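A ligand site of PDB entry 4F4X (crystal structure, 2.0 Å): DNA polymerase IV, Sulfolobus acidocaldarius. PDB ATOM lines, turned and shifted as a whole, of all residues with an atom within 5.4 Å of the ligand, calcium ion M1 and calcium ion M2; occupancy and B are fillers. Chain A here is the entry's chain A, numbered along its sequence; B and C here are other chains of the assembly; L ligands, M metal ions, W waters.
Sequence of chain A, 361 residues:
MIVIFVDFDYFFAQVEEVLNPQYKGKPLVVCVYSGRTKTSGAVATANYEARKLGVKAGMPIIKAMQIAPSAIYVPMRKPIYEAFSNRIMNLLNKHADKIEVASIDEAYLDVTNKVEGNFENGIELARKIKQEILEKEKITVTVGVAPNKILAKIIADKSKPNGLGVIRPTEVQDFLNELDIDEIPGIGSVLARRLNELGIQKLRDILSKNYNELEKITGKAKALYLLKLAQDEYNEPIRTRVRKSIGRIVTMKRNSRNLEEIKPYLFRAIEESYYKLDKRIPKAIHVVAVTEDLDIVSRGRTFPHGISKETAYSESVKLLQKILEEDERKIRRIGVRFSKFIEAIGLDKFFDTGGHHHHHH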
ATOM      1  N   ASP A   7      20.305  -3.633  13.835  1.00  0.00           N
ATOM      2  CA  ASP A   7      19.059  -4.353  13.643  1.00  0.00           C
ATOM      3  C   ASP A   7      18.169  -3.513  12.703  1.00  0.00           C
ATOM      4  O   ASP A   7      17.882  -2.360  13.008  1.00  0.00           O
ATOM      5  CB  ASP A   7      18.479  -4.555  15.050  1.00  0.00           C
ATOM      6  CG  ASP A   7      17.195  -5.298  15.067  1.00  0.00           C
ATOM      7  OD1 ASP A   7      17.029  -6.205  15.897  1.00  0.00           O
ATOM      8  OD2 ASP A   7      16.312  -4.921  14.316  1.00  0.00           O
ATOM      9  N   PHE A   8      17.765  -4.060  11.551  1.00  0.00           N
ATOM     10  CA  PHE A   8      17.107  -3.260  10.512  1.00  0.00           C
ATOM     11  C   PHE A   8      15.670  -2.950  10.879  1.00  0.00           C
ATOM     12  O   PHE A   8      14.969  -3.843  11.256  1.00  0.00           O
ATOM     13  CB  PHE A   8      17.085  -3.987   9.165  1.00  0.00           C
ATOM     14  CG  PHE A   8      18.433  -4.489   8.718  1.00  0.00           C
ATOM     15  CD1 PHE A   8      18.512  -5.552   7.837  1.00  0.00           C
ATOM     16  CD2 PHE A   8      19.604  -3.883   9.145  1.00  0.00           C
ATOM     17  CE1 PHE A   8      19.735  -6.001   7.380  1.00  0.00           C
ATOM     18  CE2 PHE A   8      20.854  -4.360   8.714  1.00  0.00           C
ATOM     19  CZ  PHE A   8      20.906  -5.416   7.830  1.00  0.00           C
ATOM     20  N   ASP A   9      15.191  -1.717  10.742  1.00  0.00           N
ATOM     21  CA  ASP A   9      13.796  -1.450  11.175  1.00  0.00           C
ATOM     22  C   ASP A   9      12.739  -2.087  10.267  1.00  0.00           C
ATOM     23  O   ASP A   9      12.853  -2.034   9.043  1.00  0.00           O
ATOM     24  CB  ASP A   9      13.530   0.060  11.278  1.00  0.00           C
ATOM     25  CG  ASP A   9      14.474   0.762  12.241  1.00  0.00           C
ATOM     26  OD1 ASP A   9      14.715   1.965  12.041  1.00  0.00           O
ATOM     27  OD2 ASP A   9      14.981   0.126  13.195  1.00  0.00           O
ATOM     28  N   TYR A  10      11.706  -2.665  10.883  1.00  0.00           N
ATOM     29  CA  TYR A  10      10.566  -3.304  10.173  1.00  0.00           C
ATOM     30  C   TYR A  10      10.952  -3.888   8.798  1.00  0.00           C
ATOM     31  O   TYR A  10      10.328  -3.614   7.786  1.00  0.00           O
ATOM     32  CB  TYR A  10       9.322  -2.360  10.101  1.00  0.00           C
ATOM     33  CG  TYR A  10       9.497  -1.053   9.326  1.00  0.00           C
ATOM     34  CD1 TYR A  10       8.906  -0.878   8.078  1.00  0.00           C
ATOM     35  CD2 TYR A  10      10.225   0.005   9.856  1.00  0.00           C
ATOM     36  CE1 TYR A  10       9.040   0.331   7.347  1.00  0.00           C
ATOM     37  CE2 TYR A  10      10.379   1.210   9.139  1.00  0.00           C
ATOM     38  CZ  TYR A  10       9.782   1.357   7.887  1.00  0.00           C
ATOM     39  OH  TYR A  10       9.920   2.532   7.187  1.00  0.00           O
ATOM     40  N   PHE A  11      11.991  -4.733   8.821  1.00  0.00           N
ATOM     41  CA  PHE A  11      12.794  -5.025   7.631  1.00  0.00           C
ATOM     42  C   PHE A  11      12.025  -5.315   6.342  1.00  0.00           C
ATOM     43  O   PHE A  11      12.149  -4.571   5.375  1.00  0.00           O
ATOM     44  CB  PHE A  11      13.830  -6.130   7.910  1.00  0.00           C
ATOM     45  CG  PHE A  11      14.849  -6.315   6.795  1.00  0.00           C
ATOM     46  CD1 PHE A  11      15.428  -5.211   6.192  1.00  0.00           C
ATOM     47  CD2 PHE A  11      15.229  -7.577   6.374  1.00  0.00           C
ATOM     48  CE1 PHE A  11      16.358  -5.347   5.152  1.00  0.00           C
ATOM     49  CE2 PHE A  11      16.153  -7.734   5.344  1.00  0.00           C
ATOM     50  CZ  PHE A  11      16.712  -6.627   4.728  1.00  0.00           C
ATOM     51  N   PHE A  12      11.241  -6.396   6.311  1.00  0.00           N
ATOM     52  CA  PHE A  12      10.615  -6.784   5.047  1.00  0.00           C
ATOM     53  C   PHE A  12       9.711  -5.672   4.513  1.00  0.00           C
ATOM     54  O   PHE A  12       9.711  -5.386   3.304  1.00  0.00           O
ATOM     55  CB  PHE A  12       9.849  -8.117   5.144  1.00  0.00           C
ATOM     56  CG  PHE A  12      10.735  -9.327   5.442  1.00  0.00           C
ATOM     57  CD1 PHE A  12      12.107  -9.200   5.601  1.00  0.00           C
ATOM     58  CD2 PHE A  12      10.179 -10.602   5.554  1.00  0.00           C
ATOM     59  CE1 PHE A  12      12.922 -10.316   5.886  1.00  0.00           C
ATOM     60  CE2 PHE A  12      10.987 -11.717   5.827  1.00  0.00           C
ATOM     61  CZ  PHE A  12      12.354 -11.554   5.980  1.00  0.00           C
ATOM     62  N   ALA A  13       8.935  -5.032   5.395  1.00  0.00           N
ATOM     63  CA  ALA A  13       8.059  -3.942   4.981  1.00  0.00           C
ATOM     64  C   ALA A  13       8.862  -2.736   4.520  1.00  0.00           C
ATOM     65  O   ALA A  13       8.460  -2.053   3.578  1.00  0.00           O
ATOM     66  CB  ALA A  13       7.045  -3.528   6.156  1.00  0.00           C
ATOM     67  N   VAL A  43       1.052 -12.984   8.670  1.00  0.00           N
ATOM     68  CA  VAL A  43       1.786 -11.729   8.550  1.00  0.00           C
ATOM     69  C   VAL A  43       3.252 -11.952   8.869  1.00  0.00           C
ATOM     70  O   VAL A  43       3.578 -12.480   9.943  1.00  0.00           O
ATOM     71  CB  VAL A  43       1.203 -10.648   9.498  1.00  0.00           C
ATOM     72  CG1 VAL A  43       2.084  -9.400   9.518  1.00  0.00           C
ATOM     73  CG2 VAL A  43      -0.244 -10.308   9.105  1.00  0.00           C
ATOM     74  N   ALA A  44       4.129 -11.594   7.930  1.00  0.00           N
ATOM     75  CA  ALA A  44       5.576 -11.718   8.148  1.00  0.00           C
ATOM     76  C   ALA A  44       6.069 -10.513   8.943  1.00  0.00           C
ATOM     77  O   ALA A  44       6.878 -10.654   9.854  1.00  0.00           O
ATOM     78  CB  ALA A  44       6.348 -11.823   6.806  1.00  0.00           C
ATOM     79  N   THR A  45       5.598  -9.324   8.581  1.00  0.00           N
ATOM     80  CA  THR A  45       5.902  -8.132   9.344  1.00  0.00           C
ATOM     81  C   THR A  45       5.000  -6.977   8.912  1.00  0.00           C
ATOM     82  O   THR A  45       4.345  -7.028   7.879  1.00  0.00           O
ATOM     83  CB  THR A  45       7.365  -7.714   9.234  1.00  0.00           C
ATOM     84  OG1 THR A  45       7.697  -6.818  10.309  1.00  0.00           O
ATOM     85  CG2 THR A  45       7.644  -7.062   7.901  1.00  0.00           C
ATOM     86  N   ALA A  46       4.947  -5.927   9.702  1.00  0.00           N
ATOM     87  CA  ALA A  46       4.107  -4.791   9.341  1.00  0.00           C
ATOM     88  C   ALA A  46       4.896  -3.556   9.643  1.00  0.00           C
ATOM     89  O   ALA A  46       5.643  -3.542  10.608  1.00  0.00           O
ATOM     90  CB  ALA A  46       2.839  -4.811  10.156  1.00  0.00           C
ATOM     91  N   TYR A  48       5.367   0.317  11.058  1.00  0.00           N
ATOM     92  CA  TYR A  48       4.901   0.866  12.331  1.00  0.00           C
ATOM     93  C   TYR A  48       3.505   1.476  12.266  1.00  0.00           C
ATOM     94  O   TYR A  48       2.762   1.388  13.232  1.00  0.00           O
ATOM     95  CB  TYR A  48       5.926   1.840  12.914  1.00  0.00           C
ATOM     96  CG  TYR A  48       7.049   1.087  13.580  1.00  0.00           C
ATOM     97  CD1 TYR A  48       7.058   0.867  14.950  1.00  0.00           C
ATOM     98  CD2 TYR A  48       8.077   0.539  12.818  1.00  0.00           C
ATOM     99  CE1 TYR A  48       8.086   0.155  15.561  1.00  0.00           C
ATOM    100  CE2 TYR A  48       9.097  -0.186  13.410  1.00  0.00           C
ATOM    101  CZ  TYR A  48       9.097  -0.382  14.767  1.00  0.00           C
ATOM    102  OH  TYR A  48      10.128  -1.094  15.345  1.00  0.00           O
ATOM    103  N   ARG A  51       1.249  -1.384  12.740  1.00  0.00           N
ATOM    104  CA  ARG A  51       1.361  -1.912  14.100  1.00  0.00           C
ATOM    105  C   ARG A  51       0.517  -1.073  15.045  1.00  0.00           C
ATOM    106  O   ARG A  51      -0.029  -1.591  16.028  1.00  0.00           O
ATOM    107  CB  ARG A  51       2.816  -1.939  14.573  1.00  0.00           C
ATOM    108  CG  ARG A  51       3.667  -2.995  13.816  1.00  0.00           C
ATOM    109  CD  ARG A  51       5.095  -3.007  14.303  1.00  0.00           C
ATOM    110  NE  ARG A  51       5.969  -3.684  13.365  1.00  0.00           N
ATOM    111  CZ  ARG A  51       7.235  -3.983  13.595  1.00  0.00           C
ATOM    112  NH1 ARG A  51       7.797  -3.659  14.758  1.00  0.00           N
ATOM    113  NH2 ARG A  51       7.957  -4.622  12.669  1.00  0.00           N
ATOM    114  N   ALA A  57       3.241  -9.471  13.616  1.00  0.00           N
ATOM    115  CA  ALA A  57       3.905 -10.607  12.951  1.00  0.00           C
ATOM    116  C   ALA A  57       3.414 -11.926  13.543  1.00  0.00           C
ATOM    117  O   ALA A  57       3.308 -12.072  14.756  1.00  0.00           O
ATOM    118  CB  ALA A  57       5.398 -10.513  13.129  1.00  0.00           C
ATOM    119  N   GLY A  58       3.095 -12.884  12.668  1.00  0.00           N
ATOM    120  CA  GLY A  58       2.601 -14.190  13.072  1.00  0.00           C
ATOM    121  C   GLY A  58       1.094 -14.301  12.917  1.00  0.00           C
ATOM    122  O   GLY A  58       0.541 -15.377  12.766  1.00  0.00           O
ATOM    123  N   MET A  76       5.048 -11.614   0.452  1.00  0.00           N
ATOM    124  CA  MET A  76       6.439 -11.675   0.816  1.00  0.00           C
ATOM    125  C   MET A  76       7.277 -12.024  -0.430  1.00  0.00           C
ATOM    126  O   MET A  76       6.901 -12.885  -1.223  1.00  0.00           O
ATOM    127  CB  MET A  76       6.650 -12.710   1.919  1.00  0.00           C
ATOM    128  CG  MET A  76       7.990 -12.550   2.645  1.00  0.00           C
ATOM    129  SD  MET A  76       8.329 -13.853   3.821  1.00  0.00           S
ATOM    130  CE  MET A  76       8.084 -15.293   2.787  1.00  0.00           C
ATOM    131  N   SER A 103      21.411 -13.031  11.611  1.00  0.00           N
ATOM    132  CA  SER A 103      20.248 -13.395  10.808  1.00  0.00           C
ATOM    133  C   SER A 103      20.171 -12.410   9.615  1.00  0.00           C
ATOM    134  O   SER A 103      21.013 -11.545   9.469  1.00  0.00           O
ATOM    135  CB  SER A 103      18.967 -13.285  11.628  1.00  0.00           C
ATOM    136  OG  SER A 103      18.572 -11.928  11.787  1.00  0.00           O
ATOM    137  N   ILE A 104      19.143 -12.552   8.791  1.00  0.00           N
ATOM    138  CA  ILE A 104      18.950 -11.710   7.618  1.00  0.00           C
ATOM    139  C   ILE A 104      18.777 -10.246   8.045  1.00  0.00           C
ATOM    140  O   ILE A 104      18.953  -9.311   7.265  1.00  0.00           O
ATOM    141  CB  ILE A 104      17.697 -12.203   6.844  1.00  0.00           C
ATOM    142  CG1 ILE A 104      17.542 -11.543   5.496  1.00  0.00           C
ATOM    143  CG2 ILE A 104      16.428 -11.986   7.641  1.00  0.00           C
ATOM    144  CD1 ILE A 104      16.242 -11.972   4.848  1.00  0.00           C
ATOM    145  N   ASP A 105      18.467 -10.059   9.316  1.00  0.00           N
ATOM    146  CA  ASP A 105      18.024  -8.779   9.847  1.00  0.00           C
ATOM    147  C   ASP A 105      19.034  -8.105  10.809  1.00  0.00           C
ATOM    148  O   ASP A 105      18.936  -6.928  11.108  1.00  0.00           O
ATOM    149  CB  ASP A 105      16.721  -9.041  10.578  1.00  0.00           C
ATOM    150  CG  ASP A 105      16.195  -7.830  11.206  1.00  0.00           C
ATOM    151  OD1 ASP A 105      16.675  -7.509  12.282  1.00  0.00           O
ATOM    152  OD2 ASP A 105      15.347  -7.155  10.601  1.00  0.00           O
ATOM    153  N   GLU A 106      20.027  -8.854  11.304  1.00  0.00           N
ATOM    154  CA  GLU A 106      20.867  -8.284  12.351  1.00  0.00           C
ATOM    155  C   GLU A 106      22.269  -8.861  12.446  1.00  0.00           C
ATOM    156  O   GLU A 106      22.524  -9.994  12.054  1.00  0.00           O
ATOM    157  CB  GLU A 106      20.150  -8.404  13.715  1.00  0.00           C
ATOM    158  CG  GLU A 106      20.229  -9.789  14.366  1.00  0.00           C
ATOM    159  CD  GLU A 106      19.323  -9.894  15.586  1.00  0.00           C
ATOM    160  OE1 GLU A 106      18.195  -9.418  15.507  1.00  0.00           O
ATOM    161  OE2 GLU A 106      19.713 -10.426  16.660  1.00  0.00           O
ATOM    162  N   LYS A 153      22.310  -5.638  22.237  1.00  0.00           N
ATOM    163  CA  LYS A 153      20.994  -5.973  21.690  1.00  0.00           C
ATOM    164  C   LYS A 153      19.837  -5.397  22.508  1.00  0.00           C
ATOM    165  O   LYS A 153      18.874  -4.886  21.946  1.00  0.00           O
ATOM    166  CB  LYS A 153      20.847  -7.489  21.547  1.00  0.00           C
ATOM    167  CG  LYS A 153      19.510  -7.923  20.980  1.00  0.00           C
ATOM    168  CD  LYS A 153      19.450  -9.455  20.881  1.00  0.00           C
ATOM    169  CE  LYS A 153      18.176  -9.936  20.212  1.00  0.00           C
ATOM    170  NZ  LYS A 153      18.092  -9.494  18.791  1.00  0.00           N
ATOM    171  N   LYS A 160      14.212   1.369  19.532  1.00  0.00           N
ATOM    172  CA  LYS A 160      13.499   1.296  18.259  1.00  0.00           C
ATOM    173  C   LYS A 160      12.336   2.291  18.138  1.00  0.00           C
ATOM    174  O   LYS A 160      11.651   2.574  19.120  1.00  0.00           O
ATOM    175  CB  LYS A 160      12.989  -0.127  18.010  1.00  0.00           C
ATOM    176  CG  LYS A 160      14.109  -1.153  17.948  1.00  0.00           C
ATOM    177  CD  LYS A 160      13.694  -2.365  17.154  1.00  0.00           C
ATOM    178  CE  LYS A 160      13.715  -2.050  15.690  1.00  0.00           C
ATOM    179  NZ  LYS A 160      14.893  -2.610  14.941  1.00  0.00           N
ATOM    180  P    DG B  13      11.181 -13.513  18.700  1.00  0.00           P
ATOM    181  OP1  DG B  13      12.075 -13.413  19.874  1.00  0.00           O
ATOM    182  OP2  DG B  13       9.934 -12.749  18.583  1.00  0.00           O
ATOM    183  O5'  DG B  13      12.061 -13.142  17.403  1.00  0.00           O
ATOM    184  C5'  DG B  13      13.274 -13.867  17.159  1.00  0.00           C
ATOM    185  C4'  DG B  13      13.598 -14.007  15.675  1.00  0.00           C
ATOM    186  O4'  DG B  13      12.806 -15.013  15.010  1.00  0.00           O
ATOM    187  C3'  DG B  13      13.387 -12.809  14.768  1.00  0.00           C
ATOM    188  O3'  DG B  13      14.312 -13.047  13.755  1.00  0.00           O
ATOM    189  C2'  DG B  13      11.955 -12.972  14.261  1.00  0.00           C
ATOM    190  C1'  DG B  13      12.041 -14.453  13.955  1.00  0.00           C
ATOM    191  N9   DG B  13      10.809 -15.206  14.033  1.00  0.00           N
ATOM    192  C8   DG B  13       9.995 -15.331  15.137  1.00  0.00           C
ATOM    193  N7   DG B  13       8.963 -16.106  14.927  1.00  0.00           N
ATOM    194  C5   DG B  13       9.135 -16.529  13.600  1.00  0.00           C
ATOM    195  C6   DG B  13       8.349 -17.397  12.813  1.00  0.00           C
ATOM    196  O6   DG B  13       7.302 -17.977  13.152  1.00  0.00           O
ATOM    197  N1   DG B  13       8.870 -17.561  11.516  1.00  0.00           N
ATOM    198  C2   DG B  13      10.034 -16.991  11.048  1.00  0.00           C
ATOM    199  N2   DG B  13      10.382 -17.265   9.775  1.00  0.00           N
ATOM    200  N3   DG B  13      10.775 -16.178  11.788  1.00  0.00           N
ATOM    201  C4   DG B  13      10.276 -15.995  13.041  1.00  0.00           C
ATOM    202  P    DC B  14      15.548 -12.058  13.602  1.00  0.00           P
ATOM    203  OP1  DC B  14      15.077 -10.760  13.989  1.00  0.00           O
ATOM    204  OP2  DC B  14      16.067 -12.175  12.204  1.00  0.00           O
ATOM    205  O5'  DC B  14      16.657 -12.656  14.605  1.00  0.00           O
ATOM    206  C5'  DC B  14      16.828 -12.331  16.009  1.00  0.00           C
ATOM    207  C4'  DC B  14      17.687 -13.392  16.706  1.00  0.00           C
ATOM    208  O4'  DC B  14      16.930 -14.636  16.679  1.00  0.00           O
ATOM    209  C3'  DC B  14      19.068 -13.742  16.115  1.00  0.00           C
ATOM    210  O3'  DC B  14      20.072 -13.978  17.120  1.00  0.00           O
ATOM    211  C2'  DC B  14      18.829 -15.057  15.361  1.00  0.00           C
ATOM    212  C1'  DC B  14      17.778 -15.708  16.255  1.00  0.00           C
ATOM    213  N1   DC B  14      16.976 -16.742  15.540  1.00  0.00           N
ATOM    214  C2   DC B  14      16.826 -18.017  16.097  1.00  0.00           C
ATOM    215  O2   DC B  14      17.373 -18.249  17.194  1.00  0.00           O
ATOM    216  N3   DC B  14      16.097 -18.945  15.416  1.00  0.00           N
ATOM    217  C4   DC B  14      15.534 -18.622  14.248  1.00  0.00           C
ATOM    218  N4   DC B  14      14.807 -19.555  13.621  1.00  0.00           N
ATOM    219  C5   DC B  14      15.654 -17.324  13.673  1.00  0.00           C
ATOM    220  C6   DC B  14      16.384 -16.429  14.338  1.00  0.00           C
ATOM    221  P    DG C   5      -2.049 -20.970   6.592  1.00  0.00           P
ATOM    222  OP1  DG C   5      -2.975 -21.130   5.449  1.00  0.00           O
ATOM    223  OP2  DG C   5      -1.644 -22.121   7.403  1.00  0.00           O
ATOM    224  O5'  DG C   5      -0.772 -20.217   5.988  1.00  0.00           O
ATOM    225  C5'  DG C   5       0.185 -19.622   6.843  1.00  0.00           C
ATOM    226  C4'  DG C   5       1.361 -19.307   5.954  1.00  0.00           C
ATOM    227  O4'  DG C   5       2.314 -18.455   6.620  1.00  0.00           O
ATOM    228  C3'  DG C   5       2.118 -20.601   5.639  1.00  0.00           C
ATOM    229  O3'  DG C   5       2.689 -20.419   4.378  1.00  0.00           O
ATOM    230  C2'  DG C   5       3.102 -20.687   6.794  1.00  0.00           C
ATOM    231  C1'  DG C   5       3.469 -19.214   6.971  1.00  0.00           C
ATOM    232  N9   DG C   5       3.709 -18.682   8.299  1.00  0.00           N
ATOM    233  C8   DG C   5       2.997 -18.952   9.441  1.00  0.00           C
ATOM    234  N7   DG C   5       3.440 -18.280  10.470  1.00  0.00           N
ATOM    235  C5   DG C   5       4.481 -17.497   9.982  1.00  0.00           C
ATOM    236  C6   DG C   5       5.315 -16.540  10.619  1.00  0.00           C
ATOM    237  O6   DG C   5       5.313 -16.188  11.808  1.00  0.00           O
ATOM    238  N1   DG C   5       6.232 -15.956   9.744  1.00  0.00           N
ATOM    239  C2   DG C   5       6.356 -16.273   8.416  1.00  0.00           C
ATOM    240  N2   DG C   5       7.317 -15.621   7.732  1.00  0.00           N
ATOM    241  N3   DG C   5       5.559 -17.157   7.800  1.00  0.00           N
ATOM    242  C4   DG C   5       4.649 -17.724   8.640  1.00  0.00           C
ATOM    243  P    DC C   6       3.485 -21.623   3.672  1.00  0.00           P
ATOM    244  OP1  DC C   6       3.442 -21.391   2.234  1.00  0.00           O
ATOM    245  OP2  DC C   6       3.010 -22.908   4.273  1.00  0.00           O
ATOM    246  O5'  DC C   6       4.966 -21.436   4.179  1.00  0.00           O
ATOM    247  C5'  DC C   6       5.778 -20.546   3.424  1.00  0.00           C
ATOM    248  C4'  DC C   6       7.080 -20.496   4.201  1.00  0.00           C
ATOM    249  O4'  DC C   6       6.775 -20.073   5.546  1.00  0.00           O
ATOM    250  C3'  DC C   6       7.860 -21.807   4.348  1.00  0.00           C
ATOM    251  O3'  DC C   6       9.106 -21.515   3.779  1.00  0.00           O
ATOM    252  C2'  DC C   6       8.042 -21.957   5.844  1.00  0.00           C
ATOM    253  C1'  DC C   6       7.824 -20.539   6.342  1.00  0.00           C
ATOM    254  N1   DC C   6       7.381 -20.434   7.750  1.00  0.00           N
ATOM    255  C2   DC C   6       8.019 -19.520   8.610  1.00  0.00           C
ATOM    256  O2   DC C   6       8.939 -18.795   8.182  1.00  0.00           O
ATOM    257  N3   DC C   6       7.582 -19.432   9.896  1.00  0.00           N
ATOM    258  C4   DC C   6       6.585 -20.211  10.316  1.00  0.00           C
ATOM    259  N4   DC C   6       6.205 -20.103  11.590  1.00  0.00           N
ATOM    260  C5   DC C   6       5.938 -21.158   9.460  1.00  0.00           C
ATOM    261  C6   DC C   6       6.364 -21.223   8.194  1.00  0.00           C
HETATM  262  N1  LIG L   1       9.819 -12.367  10.484  1.00  0.00           N
HETATM  263  C1  LIG L   1       8.982 -13.307  10.014  1.00  0.00           C
HETATM  264  N2  LIG L   1       8.034 -13.874  10.778  1.00  0.00           N
HETATM  265  C2  LIG L   1       7.892 -13.493  12.067  1.00  0.00           C
HETATM  266  C3  LIG L   1       8.714 -12.506  12.591  1.00  0.00           C
HETATM  267  C4  LIG L   1       9.691 -11.931  11.758  1.00  0.00           C
HETATM  268  O1  LIG L   1       9.126 -13.705   8.740  1.00  0.00           O
HETATM  269  N3  LIG L   1       6.873 -14.066  12.881  1.00  0.00           N
HETATM  270  C5  LIG L   1      10.824 -11.752   9.597  1.00  0.00           C
HETATM  271  C6  LIG L   1      10.269 -10.503   9.033  1.00  0.00           C
HETATM  272  C7  LIG L   1      10.890  -9.422   9.860  1.00  0.00           C
HETATM  273  C8  LIG L   1      12.208  -9.957  10.027  1.00  0.00           C
HETATM  274  O2  LIG L   1      11.949 -11.360  10.317  1.00  0.00           O
HETATM  275  O3  LIG L   1      10.890  -8.154   9.235  1.00  0.00           O
HETATM  276  C9  LIG L   1      12.901  -9.333  11.163  1.00  0.00           C
HETATM  277  O4  LIG L   1      12.375  -9.603  12.434  1.00  0.00           O
HETATM  278  P1  LIG L   1      12.177  -8.550  13.571  1.00  0.00           P
HETATM  279  O5  LIG L   1      11.978  -9.204  14.896  1.00  0.00           O
HETATM  280  O6  LIG L   1      13.444  -7.925  13.855  1.00  0.00           O
HETATM  281  O7  LIG L   1      11.009  -7.528  13.326  1.00  0.00           O
HETATM  282  P2  LIG L   1      11.013  -6.357  12.289  1.00  0.00           P
HETATM  283  O8  LIG L   1      12.241  -6.213  11.517  1.00  0.00           O
HETATM  284  O9  LIG L   1      10.031  -6.616  11.199  1.00  0.00           O
HETATM  285  O10 LIG L   1      10.600  -5.027  13.033  1.00  0.00           O
HETATM  286  P3  LIG L   1      11.416  -4.263  14.138  1.00  0.00           P
HETATM  287  O11 LIG L   1      11.614  -2.828  13.705  1.00  0.00           O
HETATM  288  O12 LIG L   1      10.648  -4.258  15.407  1.00  0.00           O
HETATM  289  O13 LIG L   1      12.812  -4.769  14.495  1.00  0.00           O
HETATM  290 CA    CA M   1      14.483  -5.781  12.765  1.00  0.00          CA
HETATM  291 CA    CA M   2      15.903  -8.451  14.689  1.00  0.00          CA
HETATM  292  O   HOH W   1       8.023  -8.522  12.338  1.00  0.00           O
HETATM  293  O   HOH W   2       9.178  -9.699  14.743  1.00  0.00           O
HETATM  294  O   HOH W   3      14.693  -8.655  16.651  1.00  0.00           O
HETATM  295  O   HOH W   4      11.090 -15.184   7.154  1.00  0.00           O
HETATM  296  O   HOH W   5       6.451 -13.242  15.621  1.00  0.00           O
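Calcium ion M2 is bound by water W3 (2.3 Å), OP1 of DC 14 of chain B (2.6 Å), the side-chain carboxylate of Glu 106 (2.6 Å), an oxygen (O6) of the ligand (2.6 Å), the side-chain carboxylate of Asp 105 (2.7 Å) and the side-chain carboxylate of Asp 7 (2.8 Å).
Calcium ion M2 has six donor atoms within binding distance.
O of Phe 8 binds calcium ion M1 (2.5 Å).
The side-chain carboxylate (OD2) of Asp 7 binds calcium ion M1.
Calcium ion M1 is bound by O8 of the ligand, 2.6 Å away.
O13 of the ligand is bound to calcium ion M1 (2.6 Å).
An oxygen (O6) of the ligand binds calcium ion M1.
OD2 of Asp 105 is bound to calcium ion M1, 2.7 Å away.
Calcium ion M1 is bound by OD1 of Asp 105, 2.8 Å away.
Along chain A the residues within 4 Å of calcium ion M2 span positions 7 to 106.
A nitrogen (N1) of the ligand lies close to the backbone carbonyl oxygen (O) of Ala 44 (3.5 Å).
CA of Asp 9 touches O11 of the ligand, at 3.6 Å.
Ala 57 touches the ligand.
N of Gly 58 touches N3 of the ligand, 3.96 Å away.
DG 13 of chain B touches the ligand (C5 to N3, 3.4 Å).
Hydrophobic or aromatic side chains within 4 Å of the ligand: Phe 11, Phe 12, Ala 44, Tyr 48 and Ala 57.
Along chain A the residues within 4 Å of the ligand span positions 7 to 160.
The backbone NH (N) of Tyr 10 is in hydrogen-bond range of an oxygen (O11) of the ligand (2.8 Å).
An oxygen (O12) of the ligand is in salt-bridge range of the guanidinium group (NH1) of Arg 51, at 3.0 Å.
OH of Tyr 48 sits at hydrogen-bond distance from O11 of the ligand, 2.8 Å away.
O6 of DG 5 of chain C sits at hydrogen-bond distance from a nitrogen (N3) of the ligand.
An oxygen (O9) of the ligand is in hydrogen-bond range of the side-chain hydroxyl of Thr 45 (2.5 Å).
O3 of the ligand sits at hydrogen-bond distance from N of Phe 12.
The side-chain amino group (NZ) of Lys 160 lies within salt-bridge range of an oxygen (O11) of the ligand, 3.5 Å away.
N of Phe 11 lies close to O8 of the ligand.
Lys 160 touches calcium ion M1 (NZ to CA, 3.9 Å).
The nearest printed residue that does not touch calcium ion M1 is Tyr 10 (4.6 Å).
OE2 of Glu 106 lies within salt-bridge range of NZ of Lys 153.
The side-chain carboxylate of Asp 7 sits close to the side-chain amino group of Lys 160 (2.8 Å).
NH2 of Arg 51 sits at hydrogen-bond distance from OG1 of Thr 45 (3.2 Å).
NE of Arg 51 sits at hydrogen-bond distance from O of Ala 46.
N of Glu 106 is in hydrogen-bond range of OG of Ser 103 (3.4 Å).
OP2 of DC 14 of chain B is in hydrogen-bond range of the side-chain hydroxyl (OG) of Ser 103, 2.6 Å away.
The side-chain amino group (NZ) of Lys 160 lies within salt-bridge range of the side-chain carboxylate (OD2) of Asp 9 (3.2 Å).
N2 of DG 13 of chain B lies close to O2 of DC 6 of chain C, at 2.6 Å.
Water W5 lies within hydrogen-bond range of N3 of the ligand (2.9 Å) and O of Ala 57 (3.5 Å).
Water W4 bridges an oxygen (O1) of the ligand and N2 of DG 13 of chain B.
Water W1 lies within hydrogen-bond range of OG1 of Thr 45 (2.7 Å), O9 of the ligand (3.0 Å) and O of Ala 44 (3.5 Å).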
